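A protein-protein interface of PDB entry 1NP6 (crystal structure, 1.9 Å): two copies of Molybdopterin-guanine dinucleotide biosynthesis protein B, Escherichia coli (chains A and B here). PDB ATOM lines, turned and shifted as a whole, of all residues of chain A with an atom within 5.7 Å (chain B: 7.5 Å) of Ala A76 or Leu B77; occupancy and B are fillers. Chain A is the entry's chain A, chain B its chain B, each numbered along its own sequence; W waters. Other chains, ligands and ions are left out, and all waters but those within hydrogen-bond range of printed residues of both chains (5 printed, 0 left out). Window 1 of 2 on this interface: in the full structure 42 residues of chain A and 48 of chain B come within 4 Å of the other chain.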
ATOM      1  N   THR A  67     -14.591   9.485 -21.938  1.00  0.00           N
ATOM      2  CA  THR A  67     -14.257   8.379 -22.846  1.00  0.00           C
ATOM      3  C   THR A  67     -14.761   8.667 -24.264  1.00  0.00           C
ATOM      4  O   THR A  67     -15.932   8.998 -24.440  1.00  0.00           O
ATOM      5  CB  THR A  67     -14.870   7.027 -22.295  1.00  0.00           C
ATOM      6  OG1 THR A  67     -14.227   6.683 -21.070  1.00  0.00           O
ATOM      7  CG2 THR A  67     -14.498   5.825 -23.170  1.00  0.00           C
ATOM      8  N   ILE A  68     -13.866   8.580 -25.255  1.00  0.00           N
ATOM      9  CA  ILE A  68     -14.264   8.566 -26.663  1.00  0.00           C
ATOM     10  C   ILE A  68     -14.179   7.138 -27.215  1.00  0.00           C
ATOM     11  O   ILE A  68     -13.189   6.435 -26.981  1.00  0.00           O
ATOM     12  CB  ILE A  68     -13.399   9.540 -27.517  1.00  0.00           C
ATOM     13  CG1 ILE A  68     -13.839  10.978 -27.283  1.00  0.00           C
ATOM     14  CG2 ILE A  68     -13.524   9.192 -29.033  1.00  0.00           C
ATOM     15  CD1 ILE A  68     -12.866  11.995 -27.831  1.00  0.00           C
ATOM     16  N   VAL A  69     -15.239   6.696 -27.891  1.00  0.00           N
ATOM     17  CA  VAL A  69     -15.263   5.377 -28.543  1.00  0.00           C
ATOM     18  C   VAL A  69     -15.574   5.611 -30.019  1.00  0.00           C
ATOM     19  O   VAL A  69     -16.602   6.206 -30.353  1.00  0.00           O
ATOM     20  CB  VAL A  69     -16.300   4.398 -27.908  1.00  0.00           C
ATOM     21  CG1 VAL A  69     -16.379   3.079 -28.703  1.00  0.00           C
ATOM     22  CG2 VAL A  69     -15.963   4.102 -26.462  1.00  0.00           C
ATOM     23  N   ALA A  70     -14.654   5.193 -30.889  1.00  0.00           N
ATOM     24  CA  ALA A  70     -14.745   5.472 -32.317  1.00  0.00           C
ATOM     25  C   ALA A  70     -14.936   4.186 -33.117  1.00  0.00           C
ATOM     26  O   ALA A  70     -14.204   3.202 -32.924  1.00  0.00           O
ATOM     27  CB  ALA A  70     -13.505   6.165 -32.774  1.00  0.00           C
ATOM     28  N   ARG A  74     -19.661   5.755 -36.815  1.00  0.00           N
ATOM     29  CA  ARG A  74     -19.917   6.844 -35.863  1.00  0.00           C
ATOM     30  C   ARG A  74     -18.938   6.831 -34.688  1.00  0.00           C
ATOM     31  O   ARG A  74     -18.279   5.810 -34.427  1.00  0.00           O
ATOM     32  CB  ARG A  74     -21.359   6.785 -35.339  1.00  0.00           C
ATOM     33  CG  ARG A  74     -21.737   5.496 -34.626  1.00  0.00           C
ATOM     34  CD  ARG A  74     -23.211   5.194 -34.723  1.00  0.00           C
ATOM     35  NE  ARG A  74     -23.365   3.765 -34.906  1.00  0.00           N
ATOM     36  CZ  ARG A  74     -24.060   3.192 -35.868  1.00  0.00           C
ATOM     37  NH1 ARG A  74     -24.728   3.911 -36.765  1.00  0.00           N
ATOM     38  NH2 ARG A  74     -24.096   1.874 -35.917  1.00  0.00           N
ATOM     39  N   TRP A  75     -18.828   7.961 -33.989  1.00  0.00           N
ATOM     40  CA  TRP A  75     -18.062   8.017 -32.731  1.00  0.00           C
ATOM     41  C   TRP A  75     -18.831   8.719 -31.594  1.00  0.00           C
ATOM     42  O   TRP A  75     -19.728   9.536 -31.850  1.00  0.00           O
ATOM     43  CB  TRP A  75     -16.654   8.623 -32.936  1.00  0.00           C
ATOM     44  CG  TRP A  75     -16.639  10.084 -33.329  1.00  0.00           C
ATOM     45  CD1 TRP A  75     -16.751  10.596 -34.603  1.00  0.00           C
ATOM     46  CD2 TRP A  75     -16.491  11.221 -32.456  1.00  0.00           C
ATOM     47  NE1 TRP A  75     -16.688  11.969 -34.570  1.00  0.00           N
ATOM     48  CE2 TRP A  75     -16.524  12.385 -33.270  1.00  0.00           C
ATOM     49  CE3 TRP A  75     -16.326  11.383 -31.066  1.00  0.00           C
ATOM     50  CZ2 TRP A  75     -16.430  13.687 -32.741  1.00  0.00           C
ATOM     51  CZ3 TRP A  75     -16.210  12.689 -30.541  1.00  0.00           C
ATOM     52  CH2 TRP A  75     -16.263  13.820 -31.381  1.00  0.00           C
ATOM     53  N   ALA A  76     -18.474   8.385 -30.352  1.00  0.00           N
ATOM     54  CA  ALA A  76     -19.157   8.902 -29.166  1.00  0.00           C
ATOM     55  C   ALA A  76     -18.203   9.528 -28.167  1.00  0.00           C
ATOM     56  O   ALA A  76     -17.069   9.044 -27.997  1.00  0.00           O
ATOM     57  CB  ALA A  76     -19.972   7.786 -28.473  1.00  0.00           C
ATOM     58  N   LEU A  77     -18.665  10.602 -27.517  1.00  0.00           N
ATOM     59  CA  LEU A  77     -17.990  11.154 -26.335  1.00  0.00           C
ATOM     60  C   LEU A  77     -18.904  10.989 -25.111  1.00  0.00           C
ATOM     61  O   LEU A  77     -20.033  11.501 -25.101  1.00  0.00           O
ATOM     62  CB  LEU A  77     -17.664  12.644 -26.519  1.00  0.00           C
ATOM     63  CG  LEU A  77     -16.968  13.551 -25.472  1.00  0.00           C
ATOM     64  CD1 LEU A  77     -17.960  14.299 -24.634  1.00  0.00           C
ATOM     65  CD2 LEU A  77     -15.927  12.872 -24.573  1.00  0.00           C
ATOM     66  N   MET A  78     -18.389  10.328 -24.084  1.00  0.00           N
ATOM     67  CA  MET A  78     -19.157  10.081 -22.851  1.00  0.00           C
ATOM     68  C   MET A  78     -18.496  10.734 -21.644  1.00  0.00           C
ATOM     69  O   MET A  78     -17.325  10.475 -21.335  1.00  0.00           O
ATOM     70  CB  MET A  78     -19.386   8.586 -22.658  1.00  0.00           C
ATOM     71  CG  MET A  78     -20.271   7.987 -23.784  1.00  0.00           C
ATOM     72  SD  MET A  78     -19.994   6.274 -24.165  1.00  0.00           S
ATOM     73  CE  MET A  78     -18.270   6.290 -24.726  1.00  0.00           C
ATOM     74  N   ARG A  95     -20.183  21.681 -27.417  1.00  0.00           N
ATOM     75  CA  ARG A  95     -19.500  20.389 -27.564  1.00  0.00           C
ATOM     76  C   ARG A  95     -19.669  19.802 -28.956  1.00  0.00           C
ATOM     77  O   ARG A  95     -18.851  18.985 -29.400  1.00  0.00           O
ATOM     78  CB  ARG A  95     -20.037  19.341 -26.576  1.00  0.00           C
ATOM     79  CG  ARG A  95     -20.020  19.753 -25.140  1.00  0.00           C
ATOM     80  CD  ARG A  95     -18.659  19.973 -24.566  1.00  0.00           C
ATOM     81  NE  ARG A  95     -18.223  21.356 -24.728  1.00  0.00           N
ATOM     82  CZ  ARG A  95     -16.959  21.751 -24.679  1.00  0.00           C
ATOM     83  NH1 ARG A  95     -15.976  20.875 -24.493  1.00  0.00           N
ATOM     84  NH2 ARG A  95     -16.666  23.038 -24.827  1.00  0.00           N
ATOM     85  N   MET A  96     -20.781  20.152 -29.598  1.00  0.00           N
ATOM     86  CA  MET A  96     -21.092  19.642 -30.929  1.00  0.00           C
ATOM     87  C   MET A  96     -20.119  20.337 -31.894  1.00  0.00           C
ATOM     88  O   MET A  96     -19.602  21.411 -31.574  1.00  0.00           O
ATOM     89  CB  MET A  96     -22.554  19.949 -31.311  1.00  0.00           C
ATOM     90  CG  MET A  96     -23.605  19.129 -30.530  1.00  0.00           C
ATOM     91  SD  MET A  96     -25.311  19.462 -31.015  1.00  0.00           S
ATOM     92  CE  MET A  96     -26.002  17.848 -31.029  1.00  0.00           C
ATOM     93  N   LEU B  39      -9.752   8.606 -21.917  1.00  0.00           N
ATOM     94  CA  LEU B  39      -9.536   7.423 -22.737  1.00  0.00           C
ATOM     95  C   LEU B  39     -10.135   7.590 -24.143  1.00  0.00           C
ATOM     96  O   LEU B  39     -11.307   7.971 -24.291  1.00  0.00           O
ATOM     97  CB  LEU B  39     -10.173   6.188 -22.101  1.00  0.00           C
ATOM     98  CG  LEU B  39     -10.020   4.852 -22.868  1.00  0.00           C
ATOM     99  CD1 LEU B  39      -8.573   4.376 -22.926  1.00  0.00           C
ATOM    100  CD2 LEU B  39     -10.874   3.777 -22.220  1.00  0.00           C
ATOM    101  N   LYS B  41     -10.639   5.160 -27.529  1.00  0.00           N
ATOM    102  CA  LYS B  41     -10.604   3.746 -27.894  1.00  0.00           C
ATOM    103  C   LYS B  41     -11.250   3.524 -29.268  1.00  0.00           C
ATOM    104  O   LYS B  41     -12.211   4.209 -29.624  1.00  0.00           O
ATOM    105  CB  LYS B  41     -11.384   2.950 -26.833  1.00  0.00           C
ATOM    106  CG  LYS B  41     -11.407   1.426 -27.015  1.00  0.00           C
ATOM    107  CD  LYS B  41     -12.210   0.735 -25.905  1.00  0.00           C
ATOM    108  CE  LYS B  41     -12.891  -0.545 -26.412  1.00  0.00           C
ATOM    109  NZ  LYS B  41     -12.024  -1.772 -26.348  1.00  0.00           N
ATOM    110  N   MET B  47     -22.199   0.402 -32.322  1.00  0.00           N
ATOM    111  CA  MET B  47     -22.476   1.292 -31.185  1.00  0.00           C
ATOM    112  C   MET B  47     -23.973   1.578 -30.933  1.00  0.00           C
ATOM    113  O   MET B  47     -24.339   2.037 -29.850  1.00  0.00           O
ATOM    114  CB  MET B  47     -21.663   2.603 -31.321  1.00  0.00           C
ATOM    115  CG  MET B  47     -20.139   2.345 -31.347  1.00  0.00           C
ATOM    116  SD  MET B  47     -19.078   3.754 -31.625  1.00  0.00           S
ATOM    117  CE  MET B  47     -19.532   4.740 -30.219  1.00  0.00           C
ATOM    118  N   PRO B  52     -24.734   4.157 -24.337  1.00  0.00           N
ATOM    119  CA  PRO B  52     -25.847   5.085 -24.607  1.00  0.00           C
ATOM    120  C   PRO B  52     -26.212   5.323 -26.090  1.00  0.00           C
ATOM    121  O   PRO B  52     -26.963   6.263 -26.382  1.00  0.00           O
ATOM    122  CB  PRO B  52     -25.324   6.391 -24.016  1.00  0.00           C
ATOM    123  CG  PRO B  52     -23.826   6.312 -24.253  1.00  0.00           C
ATOM    124  CD  PRO B  52     -23.438   4.848 -24.389  1.00  0.00           C
ATOM    125  N   GLY B  53     -25.700   4.498 -26.999  1.00  0.00           N
ATOM    126  CA  GLY B  53     -26.096   4.563 -28.399  1.00  0.00           C
ATOM    127  C   GLY B  53     -27.582   4.328 -28.595  1.00  0.00           C
ATOM    128  O   GLY B  53     -28.225   4.980 -29.417  1.00  0.00           O
ATOM    129  N   SER B  56     -30.112   7.391 -28.272  1.00  0.00           N
ATOM    130  CA  SER B  56     -30.226   8.364 -29.365  1.00  0.00           C
ATOM    131  C   SER B  56     -30.591   7.747 -30.725  1.00  0.00           C
ATOM    132  O   SER B  56     -30.655   8.467 -31.738  1.00  0.00           O
ATOM    133  CB  SER B  56     -28.933   9.194 -29.490  1.00  0.00           C
ATOM    134  OG  SER B  56     -27.819   8.417 -29.923  1.00  0.00           O
ATOM    135  N   ARG B  60     -31.387   9.702 -34.583  1.00  0.00           N
ATOM    136  CA  ARG B  60     -30.343   9.610 -35.611  1.00  0.00           C
ATOM    137  C   ARG B  60     -30.882   8.850 -36.831  1.00  0.00           C
ATOM    138  O   ARG B  60     -30.554   9.188 -37.972  1.00  0.00           O
ATOM    139  CB  ARG B  60     -29.074   8.924 -35.061  1.00  0.00           C
ATOM    140  CG  ARG B  60     -28.183   9.845 -34.230  1.00  0.00           C
ATOM    141  CD  ARG B  60     -26.917   9.189 -33.666  1.00  0.00           C
ATOM    142  NE  ARG B  60     -27.241   8.131 -32.692  1.00  0.00           N
ATOM    143  CZ  ARG B  60     -27.114   6.822 -32.929  1.00  0.00           C
ATOM    144  NH1 ARG B  60     -26.648   6.397 -34.108  1.00  0.00           N
ATOM    145  NH2 ARG B  60     -27.466   5.927 -31.990  1.00  0.00           N
ATOM    146  N   ALA B  65     -27.842  14.297 -37.236  1.00  0.00           N
ATOM    147  CA  ALA B  65     -26.453  13.956 -37.540  1.00  0.00           C
ATOM    148  C   ALA B  65     -25.534  13.953 -36.316  1.00  0.00           C
ATOM    149  O   ALA B  65     -24.535  13.229 -36.289  1.00  0.00           O
ATOM    150  CB  ALA B  65     -25.890  14.930 -38.602  1.00  0.00           C
ATOM    151  N   GLN B  66     -25.833  14.817 -35.355  1.00  0.00           N
ATOM    152  CA  GLN B  66     -25.182  14.789 -34.044  1.00  0.00           C
ATOM    153  C   GLN B  66     -26.280  14.832 -32.984  1.00  0.00           C
ATOM    154  O   GLN B  66     -27.259  15.568 -33.138  1.00  0.00           O
ATOM    155  CB  GLN B  66     -24.235  15.976 -33.860  1.00  0.00           C
ATOM    156  CG  GLN B  66     -22.917  15.899 -34.754  1.00  0.00           C
ATOM    157  CD  GLN B  66     -22.028  17.108 -34.612  1.00  0.00           C
ATOM    158  OE1 GLN B  66     -21.673  17.485 -33.504  1.00  0.00           O
ATOM    159  NE2 GLN B  66     -21.636  17.703 -35.739  1.00  0.00           N
ATOM    160  N   THR B  67     -26.126  14.021 -31.935  1.00  0.00           N
ATOM    161  CA  THR B  67     -27.065  14.050 -30.795  1.00  0.00           C
ATOM    162  C   THR B  67     -26.296  14.170 -29.491  1.00  0.00           C
ATOM    163  O   THR B  67     -25.157  13.634 -29.391  1.00  0.00           O
ATOM    164  CB  THR B  67     -27.944  12.765 -30.721  1.00  0.00           C
ATOM    165  OG1 THR B  67     -27.109  11.582 -30.727  1.00  0.00           O
ATOM    166  CG2 THR B  67     -28.821  12.622 -31.961  1.00  0.00           C
ATOM    167  N   ILE B  68     -26.932  14.846 -28.505  1.00  0.00           N
ATOM    168  CA  ILE B  68     -26.551  14.738 -27.076  1.00  0.00           C
ATOM    169  C   ILE B  68     -27.780  14.254 -26.288  1.00  0.00           C
ATOM    170  O   ILE B  68     -28.889  14.787 -26.458  1.00  0.00           O
ATOM    171  CB  ILE B  68     -25.994  16.095 -26.491  1.00  0.00           C
ATOM    172  CG1 ILE B  68     -24.609  16.423 -27.064  1.00  0.00           C
ATOM    173  CG2 ILE B  68     -25.854  16.098 -24.904  1.00  0.00           C
ATOM    174  CD1 ILE B  68     -24.126  17.837 -26.732  1.00  0.00           C
ATOM    175  N   VAL B  69     -27.561  13.251 -25.432  1.00  0.00           N
ATOM    176  CA  VAL B  69     -28.551  12.841 -24.396  1.00  0.00           C
ATOM    177  C   VAL B  69     -27.894  13.129 -23.032  1.00  0.00           C
ATOM    178  O   VAL B  69     -26.803  12.595 -22.742  1.00  0.00           O
ATOM    179  CB  VAL B  69     -28.945  11.338 -24.516  1.00  0.00           C
ATOM    180  CG1 VAL B  69     -29.974  10.944 -23.431  1.00  0.00           C
ATOM    181  CG2 VAL B  69     -29.510  11.012 -25.896  1.00  0.00           C
ATOM    182  N   TRP B  75     -23.640  12.585 -19.518  1.00  0.00           N
ATOM    183  CA  TRP B  75     -24.167  12.964 -20.834  1.00  0.00           C
ATOM    184  C   TRP B  75     -23.277  12.351 -21.933  1.00  0.00           C
ATOM    185  O   TRP B  75     -22.118  12.018 -21.669  1.00  0.00           O
ATOM    186  CB  TRP B  75     -24.349  14.496 -20.956  1.00  0.00           C
ATOM    187  CG  TRP B  75     -23.092  15.317 -20.800  1.00  0.00           C
ATOM    188  CD1 TRP B  75     -22.581  15.839 -19.641  1.00  0.00           C
ATOM    189  CD2 TRP B  75     -22.188  15.705 -21.845  1.00  0.00           C
ATOM    190  NE1 TRP B  75     -21.428  16.535 -19.905  1.00  0.00           N
ATOM    191  CE2 TRP B  75     -21.163  16.467 -21.252  1.00  0.00           C
ATOM    192  CE3 TRP B  75     -22.148  15.490 -23.231  1.00  0.00           C
ATOM    193  CZ2 TRP B  75     -20.101  17.007 -21.990  1.00  0.00           C
ATOM    194  CZ3 TRP B  75     -21.095  16.026 -23.963  1.00  0.00           C
ATOM    195  CH2 TRP B  75     -20.086  16.777 -23.340  1.00  0.00           C
ATOM    196  N   ALA B  76     -23.837  12.171 -23.137  1.00  0.00           N
ATOM    197  CA  ALA B  76     -23.171  11.467 -24.225  1.00  0.00           C
ATOM    198  C   ALA B  76     -23.425  12.185 -25.552  1.00  0.00           C
ATOM    199  O   ALA B  76     -24.565  12.512 -25.874  1.00  0.00           O
ATOM    200  CB  ALA B  76     -23.682  10.004 -24.339  1.00  0.00           C
ATOM    201  N   LEU B  77     -22.355  12.414 -26.304  1.00  0.00           N
ATOM    202  CA  LEU B  77     -22.462  12.979 -27.657  1.00  0.00           C
ATOM    203  C   LEU B  77     -22.290  11.854 -28.699  1.00  0.00           C
ATOM    204  O   LEU B  77     -21.418  10.997 -28.539  1.00  0.00           O
ATOM    205  CB  LEU B  77     -21.387  14.057 -27.819  1.00  0.00           C
ATOM    206  CG  LEU B  77     -21.173  14.523 -29.281  1.00  0.00           C
ATOM    207  CD1 LEU B  77     -22.310  15.429 -29.770  1.00  0.00           C
ATOM    208  CD2 LEU B  77     -19.817  15.215 -29.339  1.00  0.00           C
ATOM    209  N   MET B  78     -23.151  11.794 -29.722  1.00  0.00           N
ATOM    210  CA  MET B  78     -22.913  10.864 -30.817  1.00  0.00           C
ATOM    211  C   MET B  78     -22.788  11.652 -32.135  1.00  0.00           C
ATOM    212  O   MET B  78     -23.555  12.576 -32.351  1.00  0.00           O
ATOM    213  CB  MET B  78     -24.003   9.799 -30.907  1.00  0.00           C
ATOM    214  CG  MET B  78     -23.710   8.675 -31.932  1.00  0.00           C
ATOM    215  SD  MET B  78     -22.442   7.479 -31.518  1.00  0.00           S
ATOM    216  CE  MET B  78     -23.349   6.473 -30.181  1.00  0.00           C
ATOM    217  N   THR B  79     -21.808  11.282 -32.959  1.00  0.00           N
ATOM    218  CA  THR B  79     -21.555  11.916 -34.280  1.00  0.00           C
ATOM    219  C   THR B  79     -21.620  10.827 -35.356  1.00  0.00           C
ATOM    220  O   THR B  79     -20.799   9.918 -35.388  1.00  0.00           O
ATOM    221  CB  THR B  79     -20.181  12.629 -34.289  1.00  0.00           C
ATOM    222  OG1 THR B  79     -20.145  13.647 -33.274  1.00  0.00           O
ATOM    223  CG2 THR B  79     -19.943  13.428 -35.621  1.00  0.00           C
ATOM    224  N   LEU B  92      -9.890  14.251 -32.198  1.00  0.00           N
ATOM    225  CA  LEU B  92     -10.677  13.570 -31.173  1.00  0.00           C
ATOM    226  C   LEU B  92     -10.324  14.086 -29.775  1.00  0.00           C
ATOM    227  O   LEU B  92     -11.213  14.507 -29.039  1.00  0.00           O
ATOM    228  CB  LEU B  92     -10.548  12.046 -31.292  1.00  0.00           C
ATOM    229  CG  LEU B  92     -11.223  11.395 -32.506  1.00  0.00           C
ATOM    230  CD1 LEU B  92     -10.884   9.911 -32.561  1.00  0.00           C
ATOM    231  CD2 LEU B  92     -12.738  11.622 -32.533  1.00  0.00           C
ATOM    232  N   ARG B  95     -11.776  17.406 -28.828  1.00  0.00           N
ATOM    233  CA  ARG B  95     -13.220  17.477 -28.522  1.00  0.00           C
ATOM    234  C   ARG B  95     -13.498  17.115 -27.056  1.00  0.00           C
ATOM    235  O   ARG B  95     -14.614  17.328 -26.560  1.00  0.00           O
ATOM    236  CB  ARG B  95     -14.055  16.588 -29.447  1.00  0.00           C
ATOM    237  CG  ARG B  95     -13.826  16.803 -30.974  1.00  0.00           C
ATOM    238  CD  ARG B  95     -13.849  18.253 -31.437  1.00  0.00           C
ATOM    239  NE  ARG B  95     -15.175  18.869 -31.332  1.00  0.00           N
ATOM    240  CZ  ARG B  95     -15.422  20.170 -31.434  1.00  0.00           C
ATOM    241  NH1 ARG B  95     -14.429  21.027 -31.658  1.00  0.00           N
ATOM    242  NH2 ARG B  95     -16.669  20.622 -31.319  1.00  0.00           N
ATOM    243  N   MET B  96     -12.484  16.600 -26.366  1.00  0.00           N
ATOM    244  CA  MET B  96     -12.571  16.367 -24.905  1.00  0.00           C
ATOM    245  C   MET B  96     -12.476  17.684 -24.128  1.00  0.00           C
ATOM    246  O   MET B  96     -11.904  18.659 -24.634  1.00  0.00           O
ATOM    247  CB  MET B  96     -11.476  15.385 -24.439  1.00  0.00           C
ATOM    248  CG  MET B  96     -11.777  13.928 -24.796  1.00  0.00           C
ATOM    249  SD  MET B  96     -10.444  12.750 -24.417  1.00  0.00           S
ATOM    250  CE  MET B  96     -11.317  11.374 -23.913  1.00  0.00           C
HETATM  251  O   HOH W   1     -16.137  17.831 -24.091  1.00  0.00           O
HETATM  252  O   HOH W   2     -21.155   1.626 -34.557  1.00  0.00           O
HETATM  253  O   HOH W   3     -19.483  12.262 -30.909  1.00  0.00           O
HETATM  254  O   HOH W   4     -17.449  17.317 -31.146  1.00  0.00           O
HETATM  255  O   HOH W   5     -16.385  18.977 -27.785  1.00  0.00           O
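Ile A68 touches Met B96, but with the chains exchanged Met A96 does not touch Ile B68 (4.03 Å). Trp A75 touches Met B78, and with the chains exchanged Met A78 touches Trp B75. Trp A75 touches Arg B95, and with the chains exchanged Arg A95 touches Trp B75. Ala A76 touches Leu B77, and with the chains exchanged Leu A77 touches Ala B76. Of the 32 pairs that touch across the chains among the printed residues, 10 have their exchanged pair printed and touching as well.
Ile A68 touches Leu B92. CG of Met B96 touches CD1 of Ile A68 (3.8 Å). CD2 of Trp A75 touches CD2 of Leu B92, at 3.8 Å. CA of Ala A76 touches O of Leu B77, at 3.1 Å. Trp B75 touches Leu A77. O of Leu A77 touches CA of Ala B76 (3.3 Å). Pro B52 touches Met A78. CA of Met A78 touches O of Trp B75, at 3.7 Å. Trp B75 touches Arg A95 (CH2 to CG, 3.5 Å). CD2 of Leu B77 touches O of Arg A95, at 3.9 Å.
Water W5 lies within hydrogen-bond range of the backbone carbonyl oxygen (O) of Arg B95 and the backbone carbonyl oxygen (O) of Arg A95. Water W2 bridges N of Met B47 (2.8 Å) and NE of Arg A74 (3.1 Å). Water W4 bridges the guanidinium group (NE) of Arg B95 (2.8 Å) and the backbone carbonyl oxygen (O) of Arg A95 (2.8 Å). Water W3 lies within hydrogen-bond range of the side-chain hydroxyl of Thr B79 (2.8 Å), the backbone carbonyl oxygen of Trp A75 (2.9 Å) and the backbone carbonyl oxygen of Leu B77 (3.3 Å). Water W1 lies within hydrogen-bond range of O of Arg B95 (2.9 Å) and NH1 of Arg A95 (3.1 Å).
O of Thr A67 is in hydrogen-bond range of N of Met A78 (2.8 Å). The backbone NH of Ala B76 sits at hydrogen-bond distance from the backbone carbonyl oxygen of Val B69, at 3.0 Å. The side-chain hydroxyl (OG) of Ser B56 sits close to the side-chain hydroxyl (OG1) of Thr B67 (3.3 Å). OG of Ser B56 is in hydrogen-bond range of NE of Arg B60, 2.8 Å away. The backbone carbonyl oxygen (O) of Val A69 is in hydrogen-bond range of the backbone NH (N) of Ala A76, 2.9 Å away. The backbone NH of Met B78 lies within hydrogen-bond range of the backbone carbonyl oxygen of Thr B67 (2.7 Å).
Of the printed residues of chain B, Val A69 touches Lys B41 and Met B47. Of the printed residues of chain B, Arg A74 touches Met B47 (3.6 Å), Arg B60 (3.7 Å), Met B78 (3.8 Å) and Thr B79 (3.2 Å). Ala A76 touches three residues of chain B. Printed residues of chain A within 4 Å of Lys B41: Ile A68 (2.9 Å), Val A69 (3.4 Å) and Ala A70 (2.9 Å). Of the printed residues of chain A, Pro B52 touches Met A78. Of the printed residues of chain A, Arg B60 touches Arg A74. Ala B65 touches none of the printed residues of chain A. Printed residues of chain A within 4 Å of Leu B77: Trp A75 (3.99 Å), Ala A76 (3.1 Å), Leu A77 (2.8 Å), Arg A95 (3.9 Å) and Met A96 (3.99 Å).
Of the 11 printed residues of chain A, 11 touch a printed residue of chain B. Hydrophobic or aromatic side chains of chain A within 4 Å of the printed part of chain B: Ile A68, Val A69, Ala A70, Trp A75, Ala A76, Leu A77, Met A78 and Met A96. Of the 20 printed residues of chain B, 15 touch a printed residue of chain A. Printed residues of chain B that touch a printed residue of chain A: Leu B39, Lys B41, Met B47, Pro B52, Arg B60, Gln B66, Thr B67, Trp B75, Ala B76, Leu B77, Met B78, Thr B79, Leu B92, Arg B95 and Met B96. Hydrophobic or aromatic side chains of chain B that line the printed part of chain A: Met B47, Pro B52, Trp B75, Leu B77, Met B78, Leu B92 and Met B96. Among the printed residues, 32 pairs touch across the chains.
The backbone NH (N) of Lys B41 sits at hydrogen-bond distance from the backbone carbonyl oxygen (O) of Ile A68, 2.9 Å away. O of Leu B39 lies within hydrogen-bond range of N of Ile A68 (2.8 Å). The backbone carbonyl oxygen of Trp A75 sits close to the side-chain sulfur of Met B78 (3.4 Å). The side-chain sulfur of Met B47 sits close to the backbone carbonyl oxygen of Arg A74, 3.6 Å away. The backbone carbonyl oxygen (O) of Leu A77 is in hydrogen-bond range of the backbone NH (N) of Leu B77 (2.8 Å). The backbone NH of Ala A70 is in hydrogen-bond range of the backbone carbonyl oxygen of Lys B41, 2.9 Å away. The backbone NH (N) of Thr B79 sits at hydrogen-bond distance from the backbone carbonyl oxygen (O) of Trp A75 (2.9 Å). The backbone carbonyl oxygen (O) of Val A69 lies close to the side-chain sulfur (SD) of Met B47 (3.7 Å). The guanidinium group of Arg B95 sits at hydrogen-bond distance from the backbone carbonyl oxygen of Met A96. O of Arg A95 lies within hydrogen-bond range of NH2 of Arg B95 (3.3 Å).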
